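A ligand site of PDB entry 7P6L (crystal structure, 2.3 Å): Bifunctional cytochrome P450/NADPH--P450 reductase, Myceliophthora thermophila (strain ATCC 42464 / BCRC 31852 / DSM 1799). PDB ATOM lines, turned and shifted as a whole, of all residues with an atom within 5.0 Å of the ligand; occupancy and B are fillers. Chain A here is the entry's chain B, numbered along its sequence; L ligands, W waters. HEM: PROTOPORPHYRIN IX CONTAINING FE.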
ATOM      1  N   LYS A  75      -8.229  20.977   2.503  1.00  0.00           N
ATOM      2  CA  LYS A  75      -8.799  21.313   1.189  1.00  0.00           C
ATOM      3  C   LYS A  75      -7.995  22.474   0.620  1.00  0.00           C
ATOM      4  O   LYS A  75      -7.896  23.527   1.259  1.00  0.00           O
ATOM      5  CB  LYS A  75     -10.250  21.765   1.281  1.00  0.00           C
ATOM      6  CG  LYS A  75     -10.939  22.024  -0.049  1.00  0.00           C
ATOM      7  CD  LYS A  75     -12.405  22.429   0.100  1.00  0.00           C
ATOM      8  CE  LYS A  75     -12.999  22.933  -1.191  1.00  0.00           C
ATOM      9  NZ  LYS A  75     -14.475  22.798  -1.183  1.00  0.00           N
ATOM     10  N   LEU A  81     -11.924  23.067  -8.994  1.00  0.00           N
ATOM     11  CA  LEU A  81     -12.497  23.973  -7.970  1.00  0.00           C
ATOM     12  C   LEU A  81     -11.842  25.334  -8.095  1.00  0.00           C
ATOM     13  O   LEU A  81     -12.559  26.363  -7.944  1.00  0.00           O
ATOM     14  CB  LEU A  81     -12.276  23.378  -6.578  1.00  0.00           C
ATOM     15  CG  LEU A  81     -13.403  22.506  -6.039  1.00  0.00           C
ATOM     16  CD1 LEU A  81     -13.318  22.348  -4.526  1.00  0.00           C
ATOM     17  CD2 LEU A  81     -14.740  23.140  -6.424  1.00  0.00           C
ATOM     18  N   LEU A  92     -18.324  30.146   0.010  1.00  0.00           N
ATOM     19  CA  LEU A  92     -18.048  29.147   1.071  1.00  0.00           C
ATOM     20  C   LEU A  92     -17.334  27.915   0.485  1.00  0.00           C
ATOM     21  O   LEU A  92     -16.438  27.357   1.183  1.00  0.00           O
ATOM     22  CB  LEU A  92     -19.398  28.824   1.698  1.00  0.00           C
ATOM     23  CG  LEU A  92     -19.363  27.997   2.971  1.00  0.00           C
ATOM     24  CD1 LEU A  92     -18.348  28.539   3.962  1.00  0.00           C
ATOM     25  CD2 LEU A  92     -20.755  27.973   3.590  1.00  0.00           C
ATOM     26  N   PHE A  93     -17.670  27.530  -0.750  1.00  0.00           N
ATOM     27  CA  PHE A  93     -17.193  26.258  -1.381  1.00  0.00           C
ATOM     28  C   PHE A  93     -15.767  26.393  -1.931  1.00  0.00           C
ATOM     29  O   PHE A  93     -15.062  25.367  -2.011  1.00  0.00           O
ATOM     30  CB  PHE A  93     -18.129  25.819  -2.514  1.00  0.00           C
ATOM     31  CG  PHE A  93     -18.183  24.332  -2.794  1.00  0.00           C
ATOM     32  CD1 PHE A  93     -17.219  23.708  -3.575  1.00  0.00           C
ATOM     33  CD2 PHE A  93     -19.232  23.557  -2.308  1.00  0.00           C
ATOM     34  CE1 PHE A  93     -17.271  22.341  -3.826  1.00  0.00           C
ATOM     35  CE2 PHE A  93     -19.304  22.197  -2.559  1.00  0.00           C
ATOM     36  CZ  PHE A  93     -18.324  21.595  -3.338  1.00  0.00           C
ATOM     37  N   TRP A 102     -13.862  32.736   4.106  1.00  0.00           N
ATOM     38  CA  TRP A 102     -14.349  31.375   4.434  1.00  0.00           C
ATOM     39  C   TRP A 102     -15.019  31.432   5.806  1.00  0.00           C
ATOM     40  O   TRP A 102     -16.191  31.061   5.920  1.00  0.00           O
ATOM     41  CB  TRP A 102     -13.262  30.290   4.392  1.00  0.00           C
ATOM     42  CG  TRP A 102     -13.878  28.981   4.732  1.00  0.00           C
ATOM     43  CD1 TRP A 102     -14.664  28.228   3.898  1.00  0.00           C
ATOM     44  CD2 TRP A 102     -13.976  28.366   6.030  1.00  0.00           C
ATOM     45  NE1 TRP A 102     -15.190  27.161   4.568  1.00  0.00           N
ATOM     46  CE2 TRP A 102     -14.799  27.224   5.879  1.00  0.00           C
ATOM     47  CE3 TRP A 102     -13.466  28.663   7.279  1.00  0.00           C
ATOM     48  CZ2 TRP A 102     -15.091  26.375   6.937  1.00  0.00           C
ATOM     49  CZ3 TRP A 102     -13.736  27.809   8.327  1.00  0.00           C
ATOM     50  CH2 TRP A 102     -14.541  26.681   8.157  1.00  0.00           C
ATOM     51  N   HIS A 106     -18.813  31.047   6.871  1.00  0.00           N
ATOM     52  CA  HIS A 106     -19.018  29.777   7.628  1.00  0.00           C
ATOM     53  C   HIS A 106     -19.801  30.066   8.916  1.00  0.00           C
ATOM     54  O   HIS A 106     -20.823  29.414   9.151  1.00  0.00           O
ATOM     55  CB  HIS A 106     -17.699  29.064   7.947  1.00  0.00           C
ATOM     56  CG  HIS A 106     -17.867  27.872   8.820  1.00  0.00           C
ATOM     57  ND1 HIS A 106     -18.490  26.709   8.379  1.00  0.00           N
ATOM     58  CD2 HIS A 106     -17.558  27.661  10.111  1.00  0.00           C
ATOM     59  CE1 HIS A 106     -18.512  25.824   9.356  1.00  0.00           C
ATOM     60  NE2 HIS A 106     -17.957  26.394  10.435  1.00  0.00           N
ATOM     61  N   PHE A 113     -28.482  25.762   9.101  1.00  0.00           N
ATOM     62  CA  PHE A 113     -28.468  24.291   8.883  1.00  0.00           C
ATOM     63  C   PHE A 113     -28.478  23.485  10.197  1.00  0.00           C
ATOM     64  O   PHE A 113     -28.316  22.223  10.176  1.00  0.00           O
ATOM     65  CB  PHE A 113     -27.258  23.932   8.014  1.00  0.00           C
ATOM     66  CG  PHE A 113     -27.342  24.546   6.644  1.00  0.00           C
ATOM     67  CD1 PHE A 113     -28.129  23.964   5.683  1.00  0.00           C
ATOM     68  CD2 PHE A 113     -26.663  25.700   6.334  1.00  0.00           C
ATOM     69  CE1 PHE A 113     -28.182  24.496   4.398  1.00  0.00           C
ATOM     70  CE2 PHE A 113     -26.750  26.255   5.070  1.00  0.00           C
ATOM     71  CZ  PHE A 113     -27.505  25.658   4.108  1.00  0.00           C
ATOM     72  N   LEU A 159     -34.410  24.037  -2.735  1.00  0.00           N
ATOM     73  CA  LEU A 159     -33.272  24.846  -2.245  1.00  0.00           C
ATOM     74  C   LEU A 159     -33.678  26.326  -2.229  1.00  0.00           C
ATOM     75  O   LEU A 159     -33.557  26.965  -1.169  1.00  0.00           O
ATOM     76  CB  LEU A 159     -32.065  24.581  -3.157  1.00  0.00           C
ATOM     77  CG  LEU A 159     -30.745  25.263  -2.796  1.00  0.00           C
ATOM     78  CD1 LEU A 159     -30.754  26.711  -3.221  1.00  0.00           C
ATOM     79  CD2 LEU A 159     -30.432  25.140  -1.318  1.00  0.00           C
ATOM     80  N   THR A 266     -23.275  29.767  -5.232  1.00  0.00           N
ATOM     81  CA  THR A 266     -22.701  28.576  -4.563  1.00  0.00           C
ATOM     82  C   THR A 266     -23.833  27.665  -4.048  1.00  0.00           C
ATOM     83  O   THR A 266     -23.815  26.452  -4.337  1.00  0.00           O
ATOM     84  CB  THR A 266     -21.762  28.995  -3.442  1.00  0.00           C
ATOM     85  OG1 THR A 266     -20.714  29.786  -3.997  1.00  0.00           O
ATOM     86  CG2 THR A 266     -21.161  27.816  -2.732  1.00  0.00           C
ATOM     87  N   PHE A 267     -24.776  28.223  -3.292  1.00  0.00           N
ATOM     88  CA  PHE A 267     -25.886  27.431  -2.698  1.00  0.00           C
ATOM     89  C   PHE A 267     -26.880  26.970  -3.782  1.00  0.00           C
ATOM     90  O   PHE A 267     -27.316  25.847  -3.698  1.00  0.00           O
ATOM     91  CB  PHE A 267     -26.551  28.182  -1.544  1.00  0.00           C
ATOM     92  CG  PHE A 267     -25.769  28.061  -0.254  1.00  0.00           C
ATOM     93  CD1 PHE A 267     -25.940  26.962   0.577  1.00  0.00           C
ATOM     94  CD2 PHE A 267     -24.807  28.987   0.073  1.00  0.00           C
ATOM     95  CE1 PHE A 267     -25.226  26.839   1.756  1.00  0.00           C
ATOM     96  CE2 PHE A 267     -24.082  28.855   1.252  1.00  0.00           C
ATOM     97  CZ  PHE A 267     -24.287  27.782   2.084  1.00  0.00           C
ATOM     98  N   ALA A 270     -24.462  23.922  -5.381  1.00  0.00           N
ATOM     99  CA  ALA A 270     -24.152  22.899  -4.351  1.00  0.00           C
ATOM    100  C   ALA A 270     -25.436  22.402  -3.696  1.00  0.00           C
ATOM    101  O   ALA A 270     -25.471  21.248  -3.230  1.00  0.00           O
ATOM    102  CB  ALA A 270     -23.203  23.479  -3.328  1.00  0.00           C
ATOM    103  N   GLY A 271     -26.442  23.272  -3.600  1.00  0.00           N
ATOM    104  CA  GLY A 271     -27.672  23.007  -2.827  1.00  0.00           C
ATOM    105  C   GLY A 271     -28.729  22.242  -3.624  1.00  0.00           C
ATOM    106  O   GLY A 271     -29.805  21.993  -3.039  1.00  0.00           O
ATOM    107  N   THR A 274     -26.206  18.007  -6.523  1.00  0.00           N
ATOM    108  CA  THR A 274     -25.743  16.689  -6.005  1.00  0.00           C
ATOM    109  C   THR A 274     -26.948  15.926  -5.439  1.00  0.00           C
ATOM    110  O   THR A 274     -26.948  14.678  -5.551  1.00  0.00           O
ATOM    111  CB  THR A 274     -24.552  16.854  -5.051  1.00  0.00           C
ATOM    112  OG1 THR A 274     -24.801  17.817  -4.029  1.00  0.00           O
ATOM    113  CG2 THR A 274     -23.330  17.309  -5.809  1.00  0.00           C
ATOM    114  N   THR A 275     -27.966  16.610  -4.895  1.00  0.00           N
ATOM    115  CA  THR A 275     -29.207  15.980  -4.430  1.00  0.00           C
ATOM    116  C   THR A 275     -30.007  15.444  -5.619  1.00  0.00           C
ATOM    117  O   THR A 275     -30.625  14.382  -5.482  1.00  0.00           O
ATOM    118  CB  THR A 275     -30.018  16.934  -3.554  1.00  0.00           C
ATOM    119  OG1 THR A 275     -29.125  17.491  -2.603  1.00  0.00           O
ATOM    120  CG2 THR A 275     -31.131  16.223  -2.823  1.00  0.00           C
ATOM    121  N   LEU A 278     -28.330  12.251  -6.432  1.00  0.00           N
ATOM    122  CA  LEU A 278     -28.582  11.199  -5.419  1.00  0.00           C
ATOM    123  C   LEU A 278     -29.893  10.527  -5.770  1.00  0.00           C
ATOM    124  O   LEU A 278     -29.894   9.299  -6.011  1.00  0.00           O
ATOM    125  CB  LEU A 278     -28.636  11.819  -4.020  1.00  0.00           C
ATOM    126  CG  LEU A 278     -29.099  10.890  -2.889  1.00  0.00           C
ATOM    127  CD1 LEU A 278     -28.297   9.598  -2.887  1.00  0.00           C
ATOM    128  CD2 LEU A 278     -28.994  11.598  -1.542  1.00  0.00           C
ATOM    129  N   LEU A 328     -24.967   6.610  -2.369  1.00  0.00           N
ATOM    130  CA  LEU A 328     -23.823   7.568  -2.249  1.00  0.00           C
ATOM    131  C   LEU A 328     -22.502   6.800  -2.155  1.00  0.00           C
ATOM    132  O   LEU A 328     -21.486   7.371  -2.536  1.00  0.00           O
ATOM    133  CB  LEU A 328     -24.006   8.465  -1.021  1.00  0.00           C
ATOM    134  CG  LEU A 328     -25.044   9.590  -1.157  1.00  0.00           C
ATOM    135  CD1 LEU A 328     -25.097  10.423   0.107  1.00  0.00           C
ATOM    136  CD2 LEU A 328     -24.725  10.474  -2.363  1.00  0.00           C
ATOM    137  N   THR A 333     -21.902  11.727  -5.738  1.00  0.00           N
ATOM    138  CA  THR A 333     -22.314  12.629  -6.848  1.00  0.00           C
ATOM    139  C   THR A 333     -21.292  13.757  -6.957  1.00  0.00           C
ATOM    140  O   THR A 333     -21.262  14.386  -8.024  1.00  0.00           O
ATOM    141  CB  THR A 333     -23.766  13.075  -6.686  1.00  0.00           C
ATOM    142  OG1 THR A 333     -23.917  13.461  -5.335  1.00  0.00           O
ATOM    143  CG2 THR A 333     -24.754  11.984  -7.045  1.00  0.00           C
ATOM    144  N   ILE A 334     -20.508  13.997  -5.901  1.00  0.00           N
ATOM    145  CA  ILE A 334     -19.120  14.553  -6.029  1.00  0.00           C
ATOM    146  C   ILE A 334     -18.157  13.383  -5.847  1.00  0.00           C
ATOM    147  O   ILE A 334     -17.986  12.890  -4.719  1.00  0.00           O
ATOM    148  CB  ILE A 334     -18.858  15.694  -5.040  1.00  0.00           C
ATOM    149  CG1 ILE A 334     -19.611  16.970  -5.424  1.00  0.00           C
ATOM    150  CG2 ILE A 334     -17.362  15.954  -4.919  1.00  0.00           C
ATOM    151  CD1 ILE A 334     -19.812  17.942  -4.281  1.00  0.00           C
ATOM    152  N   ILE A 337     -12.793  14.494  -3.998  1.00  0.00           N
ATOM    153  CA  ILE A 337     -12.433  15.672  -3.176  1.00  0.00           C
ATOM    154  C   ILE A 337     -10.911  15.766  -3.107  1.00  0.00           C
ATOM    155  O   ILE A 337     -10.234  14.731  -3.258  1.00  0.00           O
ATOM    156  CB  ILE A 337     -13.099  15.626  -1.781  1.00  0.00           C
ATOM    157  CG1 ILE A 337     -12.731  14.375  -0.977  1.00  0.00           C
ATOM    158  CG2 ILE A 337     -14.598  15.812  -1.899  1.00  0.00           C
ATOM    159  CD1 ILE A 337     -13.204  14.456   0.449  1.00  0.00           C
ATOM    160  N   ASN A 338     -10.391  16.973  -2.923  1.00  0.00           N
ATOM    161  CA  ASN A 338      -8.921  17.217  -2.924  1.00  0.00           C
ATOM    162  C   ASN A 338      -8.397  17.464  -1.507  1.00  0.00           C
ATOM    163  O   ASN A 338      -9.060  18.182  -0.718  1.00  0.00           O
ATOM    164  CB  ASN A 338      -8.560  18.408  -3.806  1.00  0.00           C
ATOM    165  CG  ASN A 338      -9.035  18.239  -5.226  1.00  0.00           C
ATOM    166  OD1 ASN A 338      -8.929  17.152  -5.806  1.00  0.00           O
ATOM    167  ND2 ASN A 338      -9.556  19.327  -5.762  1.00  0.00           N
ATOM    168  N   LYS A 402     -17.353   8.693   2.458  1.00  0.00           N
ATOM    169  CA  LYS A 402     -17.133  10.162   2.618  1.00  0.00           C
ATOM    170  C   LYS A 402     -17.835  10.970   1.529  1.00  0.00           C
ATOM    171  O   LYS A 402     -17.270  11.949   1.034  1.00  0.00           O
ATOM    172  CB  LYS A 402     -15.619  10.383   2.606  1.00  0.00           C
ATOM    173  CG  LYS A 402     -14.852   9.752   3.759  1.00  0.00           C
ATOM    174  CD  LYS A 402     -15.210  10.312   5.101  1.00  0.00           C
ATOM    175  CE  LYS A 402     -14.535  11.626   5.374  1.00  0.00           C
ATOM    176  NZ  LYS A 402     -14.869  12.159   6.714  1.00  0.00           N
ATOM    177  N   PRO A 403     -19.103  10.702   1.148  1.00  0.00           N
ATOM    178  CA  PRO A 403     -19.716  11.384   0.010  1.00  0.00           C
ATOM    179  C   PRO A 403     -20.025  12.855   0.336  1.00  0.00           C
ATOM    180  O   PRO A 403     -20.218  13.615  -0.602  1.00  0.00           O
ATOM    181  CB  PRO A 403     -21.003  10.596  -0.219  1.00  0.00           C
ATOM    182  CG  PRO A 403     -21.377  10.136   1.178  1.00  0.00           C
ATOM    183  CD  PRO A 403     -20.045   9.786   1.825  1.00  0.00           C
ATOM    184  N   PHE A 404     -20.020  13.218   1.627  1.00  0.00           N
ATOM    185  CA  PHE A 404     -20.277  14.580   2.176  1.00  0.00           C
ATOM    186  C   PHE A 404     -18.967  15.256   2.597  1.00  0.00           C
ATOM    187  O   PHE A 404     -19.010  16.228   3.361  1.00  0.00           O
ATOM    188  CB  PHE A 404     -21.292  14.531   3.338  1.00  0.00           C
ATOM    189  CG  PHE A 404     -22.692  14.135   2.916  1.00  0.00           C
ATOM    190  CD1 PHE A 404     -23.459  15.002   2.132  1.00  0.00           C
ATOM    191  CD2 PHE A 404     -23.237  12.898   3.232  1.00  0.00           C
ATOM    192  CE1 PHE A 404     -24.735  14.656   1.695  1.00  0.00           C
ATOM    193  CE2 PHE A 404     -24.513  12.551   2.805  1.00  0.00           C
ATOM    194  CZ  PHE A 404     -25.251  13.422   2.031  1.00  0.00           C
ATOM    195  N   GLY A 405     -17.817  14.769   2.119  1.00  0.00           N
ATOM    196  CA  GLY A 405     -16.509  15.406   2.377  1.00  0.00           C
ATOM    197  C   GLY A 405     -16.067  15.234   3.822  1.00  0.00           C
ATOM    198  O   GLY A 405     -16.655  14.390   4.507  1.00  0.00           O
ATOM    199  N   MET A 408     -13.407  20.408   8.777  1.00  0.00           N
ATOM    200  CA  MET A 408     -14.130  21.692   8.896  1.00  0.00           C
ATOM    201  C   MET A 408     -14.605  22.090   7.488  1.00  0.00           C
ATOM    202  O   MET A 408     -15.507  22.957   7.414  1.00  0.00           O
ATOM    203  CB  MET A 408     -13.345  22.820   9.587  1.00  0.00           C
ATOM    204  CG  MET A 408     -11.969  23.092   9.006  1.00  0.00           C
ATOM    205  SD  MET A 408     -11.323  24.818   9.279  1.00  0.00           S
ATOM    206  CE  MET A 408     -10.640  25.197   7.658  1.00  0.00           C
ATOM    207  N   ARG A 409     -14.088  21.442   6.421  1.00  0.00           N
ATOM    208  CA  ARG A 409     -14.505  21.717   5.004  1.00  0.00           C
ATOM    209  C   ARG A 409     -15.508  20.678   4.478  1.00  0.00           C
ATOM    210  O   ARG A 409     -15.686  20.599   3.258  1.00  0.00           O
ATOM    211  CB  ARG A 409     -13.268  21.801   4.088  1.00  0.00           C
ATOM    212  CG  ARG A 409     -12.352  22.990   4.343  1.00  0.00           C
ATOM    213  CD  ARG A 409     -13.033  24.348   4.367  1.00  0.00           C
ATOM    214  NE  ARG A 409     -13.738  24.701   3.124  1.00  0.00           N
ATOM    215  CZ  ARG A 409     -13.282  25.515   2.165  1.00  0.00           C
ATOM    216  NH1 ARG A 409     -12.071  26.077   2.286  1.00  0.00           N
ATOM    217  NH2 ARG A 409     -14.030  25.797   1.107  1.00  0.00           N
ATOM    218  N   ALA A 410     -16.155  19.931   5.371  1.00  0.00           N
ATOM    219  CA  ALA A 410     -17.244  18.978   5.021  1.00  0.00           C
ATOM    220  C   ALA A 410     -18.522  19.760   4.668  1.00  0.00           C
ATOM    221  O   ALA A 410     -18.610  20.960   4.996  1.00  0.00           O
ATOM    222  CB  ALA A 410     -17.520  18.015   6.151  1.00  0.00           C
ATOM    223  N   CYS A 411     -19.462  19.072   4.038  1.00  0.00           N
ATOM    224  CA  CYS A 411     -20.753  19.609   3.536  1.00  0.00           C
ATOM    225  C   CYS A 411     -21.564  20.250   4.679  1.00  0.00           C
ATOM    226  O   CYS A 411     -21.983  19.536   5.576  1.00  0.00           O
ATOM    227  CB  CYS A 411     -21.563  18.518   2.857  1.00  0.00           C
ATOM    228  SG  CYS A 411     -23.084  19.143   2.079  1.00  0.00           S
ATOM    229  N   ILE A 412     -21.771  21.561   4.614  1.00  0.00           N
ATOM    230  CA  ILE A 412     -22.661  22.359   5.518  1.00  0.00           C
ATOM    231  C   ILE A 412     -24.125  21.961   5.286  1.00  0.00           C
ATOM    232  O   ILE A 412     -24.929  22.235   6.183  1.00  0.00           O
ATOM    233  CB  ILE A 412     -22.449  23.869   5.250  1.00  0.00           C
ATOM    234  CG1 ILE A 412     -23.029  24.736   6.372  1.00  0.00           C
ATOM    235  CG2 ILE A 412     -23.011  24.299   3.913  1.00  0.00           C
ATOM    236  CD1 ILE A 412     -22.744  26.214   6.263  1.00  0.00           C
ATOM    237  N   GLY A 413     -24.468  21.408   4.120  1.00  0.00           N
ATOM    238  CA  GLY A 413     -25.847  21.223   3.634  1.00  0.00           C
ATOM    239  C   GLY A 413     -26.366  19.814   3.857  1.00  0.00           C
ATOM    240  O   GLY A 413     -27.570  19.577   3.599  1.00  0.00           O
ATOM    241  N   ARG A 414     -25.509  18.921   4.339  1.00  0.00           N
ATOM    242  CA  ARG A 414     -25.800  17.478   4.522  1.00  0.00           C
ATOM    243  C   ARG A 414     -27.199  17.293   5.099  1.00  0.00           C
ATOM    244  O   ARG A 414     -28.019  16.610   4.500  1.00  0.00           O
ATOM    245  CB  ARG A 414     -24.716  16.851   5.417  1.00  0.00           C
ATOM    246  CG  ARG A 414     -24.720  15.326   5.485  1.00  0.00           C
ATOM    247  CD  ARG A 414     -23.982  14.889   6.702  1.00  0.00           C
ATOM    248  NE  ARG A 414     -24.179  13.483   6.968  1.00  0.00           N
ATOM    249  CZ  ARG A 414     -23.220  12.609   7.252  1.00  0.00           C
ATOM    250  NH1 ARG A 414     -21.962  12.989   7.320  1.00  0.00           N
ATOM    251  NH2 ARG A 414     -23.516  11.333   7.496  1.00  0.00           N
ATOM    252  N   PHE A 416     -29.851  19.138   5.223  1.00  0.00           N
ATOM    253  CA  PHE A 416     -30.877  19.646   4.270  1.00  0.00           C
ATOM    254  C   PHE A 416     -31.107  18.574   3.216  1.00  0.00           C
ATOM    255  O   PHE A 416     -32.249  18.105   3.072  1.00  0.00           O
ATOM    256  CB  PHE A 416     -30.418  20.963   3.649  1.00  0.00           C
ATOM    257  CG  PHE A 416     -31.443  21.666   2.790  1.00  0.00           C
ATOM    258  CD1 PHE A 416     -31.602  21.324   1.460  1.00  0.00           C
ATOM    259  CD2 PHE A 416     -32.207  22.693   3.311  1.00  0.00           C
ATOM    260  CE1 PHE A 416     -32.538  21.965   0.667  1.00  0.00           C
ATOM    261  CE2 PHE A 416     -33.145  23.343   2.529  1.00  0.00           C
ATOM    262  CZ  PHE A 416     -33.310  22.980   1.197  1.00  0.00           C
ATOM    263  N   ALA A 417     -30.046  18.170   2.533  1.00  0.00           N
ATOM    264  CA  ALA A 417     -30.074  17.095   1.511  1.00  0.00           C
ATOM    265  C   ALA A 417     -30.755  15.851   2.076  1.00  0.00           C
ATOM    266  O   ALA A 417     -31.516  15.196   1.340  1.00  0.00           O
ATOM    267  CB  ALA A 417     -28.676  16.774   1.058  1.00  0.00           C
HETATM  268  CHA HEM L   1     -19.488  20.763   0.492  1.00  0.00           C
HETATM  269  CHB HEM L   1     -21.280  16.639  -1.120  1.00  0.00           C
HETATM  270  CHC HEM L   1     -25.801  18.589  -0.751  1.00  0.00           C
HETATM  271  CHD HEM L   1     -23.801  22.819   0.248  1.00  0.00           C
HETATM  272  C1A HEM L   1     -19.608  19.469   0.085  1.00  0.00           C
HETATM  273  C2A HEM L   1     -18.483  18.637  -0.168  1.00  0.00           C
HETATM  274  C3A HEM L   1     -18.968  17.506  -0.626  1.00  0.00           C
HETATM  275  C4A HEM L   1     -20.395  17.597  -0.691  1.00  0.00           C
HETATM  276  CMA HEM L   1     -18.053  16.387  -0.972  1.00  0.00           C
HETATM  277  CAA HEM L   1     -17.006  18.878   0.032  1.00  0.00           C
HETATM  278  CBA HEM L   1     -16.243  19.491  -1.170  1.00  0.00           C
HETATM  279  CGA HEM L   1     -14.717  19.399  -1.024  1.00  0.00           C
HETATM  280  O1A HEM L   1     -13.994  20.031  -1.864  1.00  0.00           O
HETATM  281  O2A HEM L   1     -14.170  18.712  -0.098  1.00  0.00           O
HETATM  282  C1B HEM L   1     -22.707  16.800  -1.169  1.00  0.00           C
HETATM  283  C2B HEM L   1     -23.637  15.801  -1.561  1.00  0.00           C
HETATM  284  C3B HEM L   1     -24.917  16.328  -1.462  1.00  0.00           C
HETATM  285  C4B HEM L   1     -24.737  17.686  -0.970  1.00  0.00           C
HETATM  286  CMB HEM L   1     -23.260  14.428  -1.980  1.00  0.00           C
HETATM  287  CAB HEM L   1     -26.305  15.746  -1.667  1.00  0.00           C
HETATM  288  CBB HEM L   1     -26.641  14.452  -1.825  1.00  0.00           C
HETATM  289  C1C HEM L   1     -25.669  19.943  -0.430  1.00  0.00           C
HETATM  290  C2C HEM L   1     -26.704  20.840  -0.071  1.00  0.00           C
HETATM  291  C3C HEM L   1     -26.155  22.043   0.222  1.00  0.00           C
HETATM  292  C4C HEM L   1     -24.741  21.868   0.020  1.00  0.00           C
HETATM  293  CMC HEM L   1     -28.156  20.535  -0.025  1.00  0.00           C
HETATM  294  CAC HEM L   1     -26.808  23.295   0.650  1.00  0.00           C
HETATM  295  CBC HEM L   1     -28.081  23.534   0.959  1.00  0.00           C
HETATM  296  C1D HEM L   1     -22.474  22.567   0.381  1.00  0.00           C
HETATM  297  C2D HEM L   1     -21.536  23.663   0.689  1.00  0.00           C
HETATM  298  C3D HEM L   1     -20.344  23.091   0.767  1.00  0.00           C
HETATM  299  C4D HEM L   1     -20.526  21.656   0.500  1.00  0.00           C
HETATM  300  CMD HEM L   1     -21.773  25.142   0.917  1.00  0.00           C
HETATM  301  CAD HEM L   1     -19.110  23.883   1.116  1.00  0.00           C
HETATM  302  CBD HEM L   1     -18.850  23.913   2.625  1.00  0.00           C
HETATM  303  CGD HEM L   1     -17.419  24.390   2.962  1.00  0.00           C
HETATM  304  O1D HEM L   1     -16.352  23.851   2.479  1.00  0.00           O
HETATM  305  O2D HEM L   1     -17.322  25.371   3.747  1.00  0.00           O
HETATM  306  NA  HEM L   1     -20.769  18.807  -0.244  1.00  0.00           N
HETATM  307  NB  HEM L   1     -23.414  17.877  -0.815  1.00  0.00           N
HETATM  308  NC  HEM L   1     -24.469  20.588  -0.363  1.00  0.00           N
HETATM  309  ND  HEM L   1     -21.838  21.389   0.289  1.00  0.00           N
HETATM  310 FE   HEM L   1     -22.585  19.680  -0.134  1.00  0.00          FE
HETATM  311  O   HOH W   1     -14.582  18.385   2.321  1.00  0.00           O
HETATM  312  O   HOH W   2     -27.226  19.210  -3.364  1.00  0.00           O
HETATM  313  O   HOH W   3     -23.208  19.526  -2.888  1.00  0.00           O
HETATM  314  O   HOH W   4     -15.832  21.907   0.987  1.00  0.00           O
HETATM  315  O   HOH W   5     -12.143  19.159  -3.879  1.00  0.00           O
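An oxygen (O1D) of the ligand is in salt-bridge range of the guanidinium group of Arg 409 (2.8 Å). An iron atom (FE) of the ligand is bound by the side-chain sulfur (SG) of Cys 411, at 2.3 Å. NZ of Lys 75 lies within salt-bridge range of O1A of the ligand. NE1 of Trp 102 sits at hydrogen-bond distance from O2D of the ligand (2.9 Å).
The backbone NH (N) of Gly 413 lies close to the side-chain sulfur (SG) of Cys 411, at 3.3 Å. The side-chain sulfur of Cys 411 lies close to the backbone NH of Arg 414, at 3.3 Å. The guanidinium group (NH2) of Arg 409 is in hydrogen-bond range of the backbone carbonyl oxygen (O) of Phe 93 (3.3 Å). The side-chain amino group (NZ) of Lys 75 lies within hydrogen-bond range of the backbone carbonyl oxygen (O) of Phe 93. O of Phe 404 lies within hydrogen-bond range of N of Cys 411, 3.0 Å away. O of Thr 274 sits at hydrogen-bond distance from OG1 of Thr 333. The guanidinium group (NH2) of Arg 409 sits at hydrogen-bond distance from the backbone carbonyl oxygen (O) of Leu 92 (2.9 Å).
The backbone carbonyl oxygen of Leu 92 lies close to an oxygen (O2D) of the ligand. O of Ala 270 lies close to NC of the ligand (3.1 Å). Leu 81 touches the ligand. Phe 93 touches the ligand (CD2 to C3D, 3.3 Å). Phe 113 touches the ligand (CE1 to CBC, 3.6 Å). CD2 of Leu 159 touches CBC of the ligand (3.6 Å). CD1 of Phe 267 touches CAC of the ligand (3.8 Å). CA of Gly 271 touches C3C of the ligand, 3.5 Å away. OG1 of Thr 274 touches C3B of the ligand (3.0 Å). OG1 of Thr 275 touches CAB of the ligand, at 3.4 Å. Leu 278 touches the ligand. Thr 333 touches the ligand. Ile 334 touches the ligand. CG2 of Ile 337 touches O2A of the ligand (3.4 Å). Pro 403 touches the ligand (O to CHB, 3.2 Å). Phe 404 touches the ligand (CE1 to C3B, 3.6 Å). Gly 405 touches the ligand. Ala 410 touches the ligand (O to CBD, 3.8 Å). CG2 of Ile 412 touches CMD of the ligand, 3.3 Å away. Gly 413 touches the ligand. Phe 416 touches the ligand. Ala 417 touches the ligand. Hydrophobic or aromatic side chains within 4 Å of the ligand: Leu 81, Leu 92, Phe 93, Trp 102, Phe 113, Leu 159, Phe 267, Ala 270, Leu 278, Ile 334, Ile 337, Phe 404, Ile 412, Phe 416 and Ala 417. 26 residues have an atom within 4 Å of the ligand: Lys 75, Leu 81, Leu 92, Phe 93, Trp 102, Phe 113, Leu 159, Phe 267, Ala 270, Gly 271, Thr 274, Thr 275, Leu 278, Thr 333, Ile 334, Ile 337, Pro 403, Phe 404, Gly 405, Arg 409, Ala 410, Cys 411, Ile 412, Gly 413, Phe 416 and Ala 417. The nearest printed residue that does not touch the ligand is Leu 328 (4.2 Å).
Water W1 lies within hydrogen-bond range of an oxygen (O2A) of the ligand and the backbone carbonyl oxygen of Arg 409. Water W4 lies within hydrogen-bond range of an oxygen (O1D) of the ligand (2.5 Å), the backbone carbonyl oxygen of Arg 409 (2.6 Å) and the side-chain amino group of Lys 75 (2.7 Å). Water W3 lies within hydrogen-bond range of the side-chain hydroxyl of Thr 274 (2.6 Å) and the backbone carbonyl oxygen of Ala 270 (2.9 Å). Water W5 lies within hydrogen-bond range of O1A of the ligand (2.9 Å) and N of Asn 338 (3.0 Å). Water W2 lies within hydrogen-bond range of OG1 of Thr 275, O of Ala 270 and OG1 of Thr 274.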
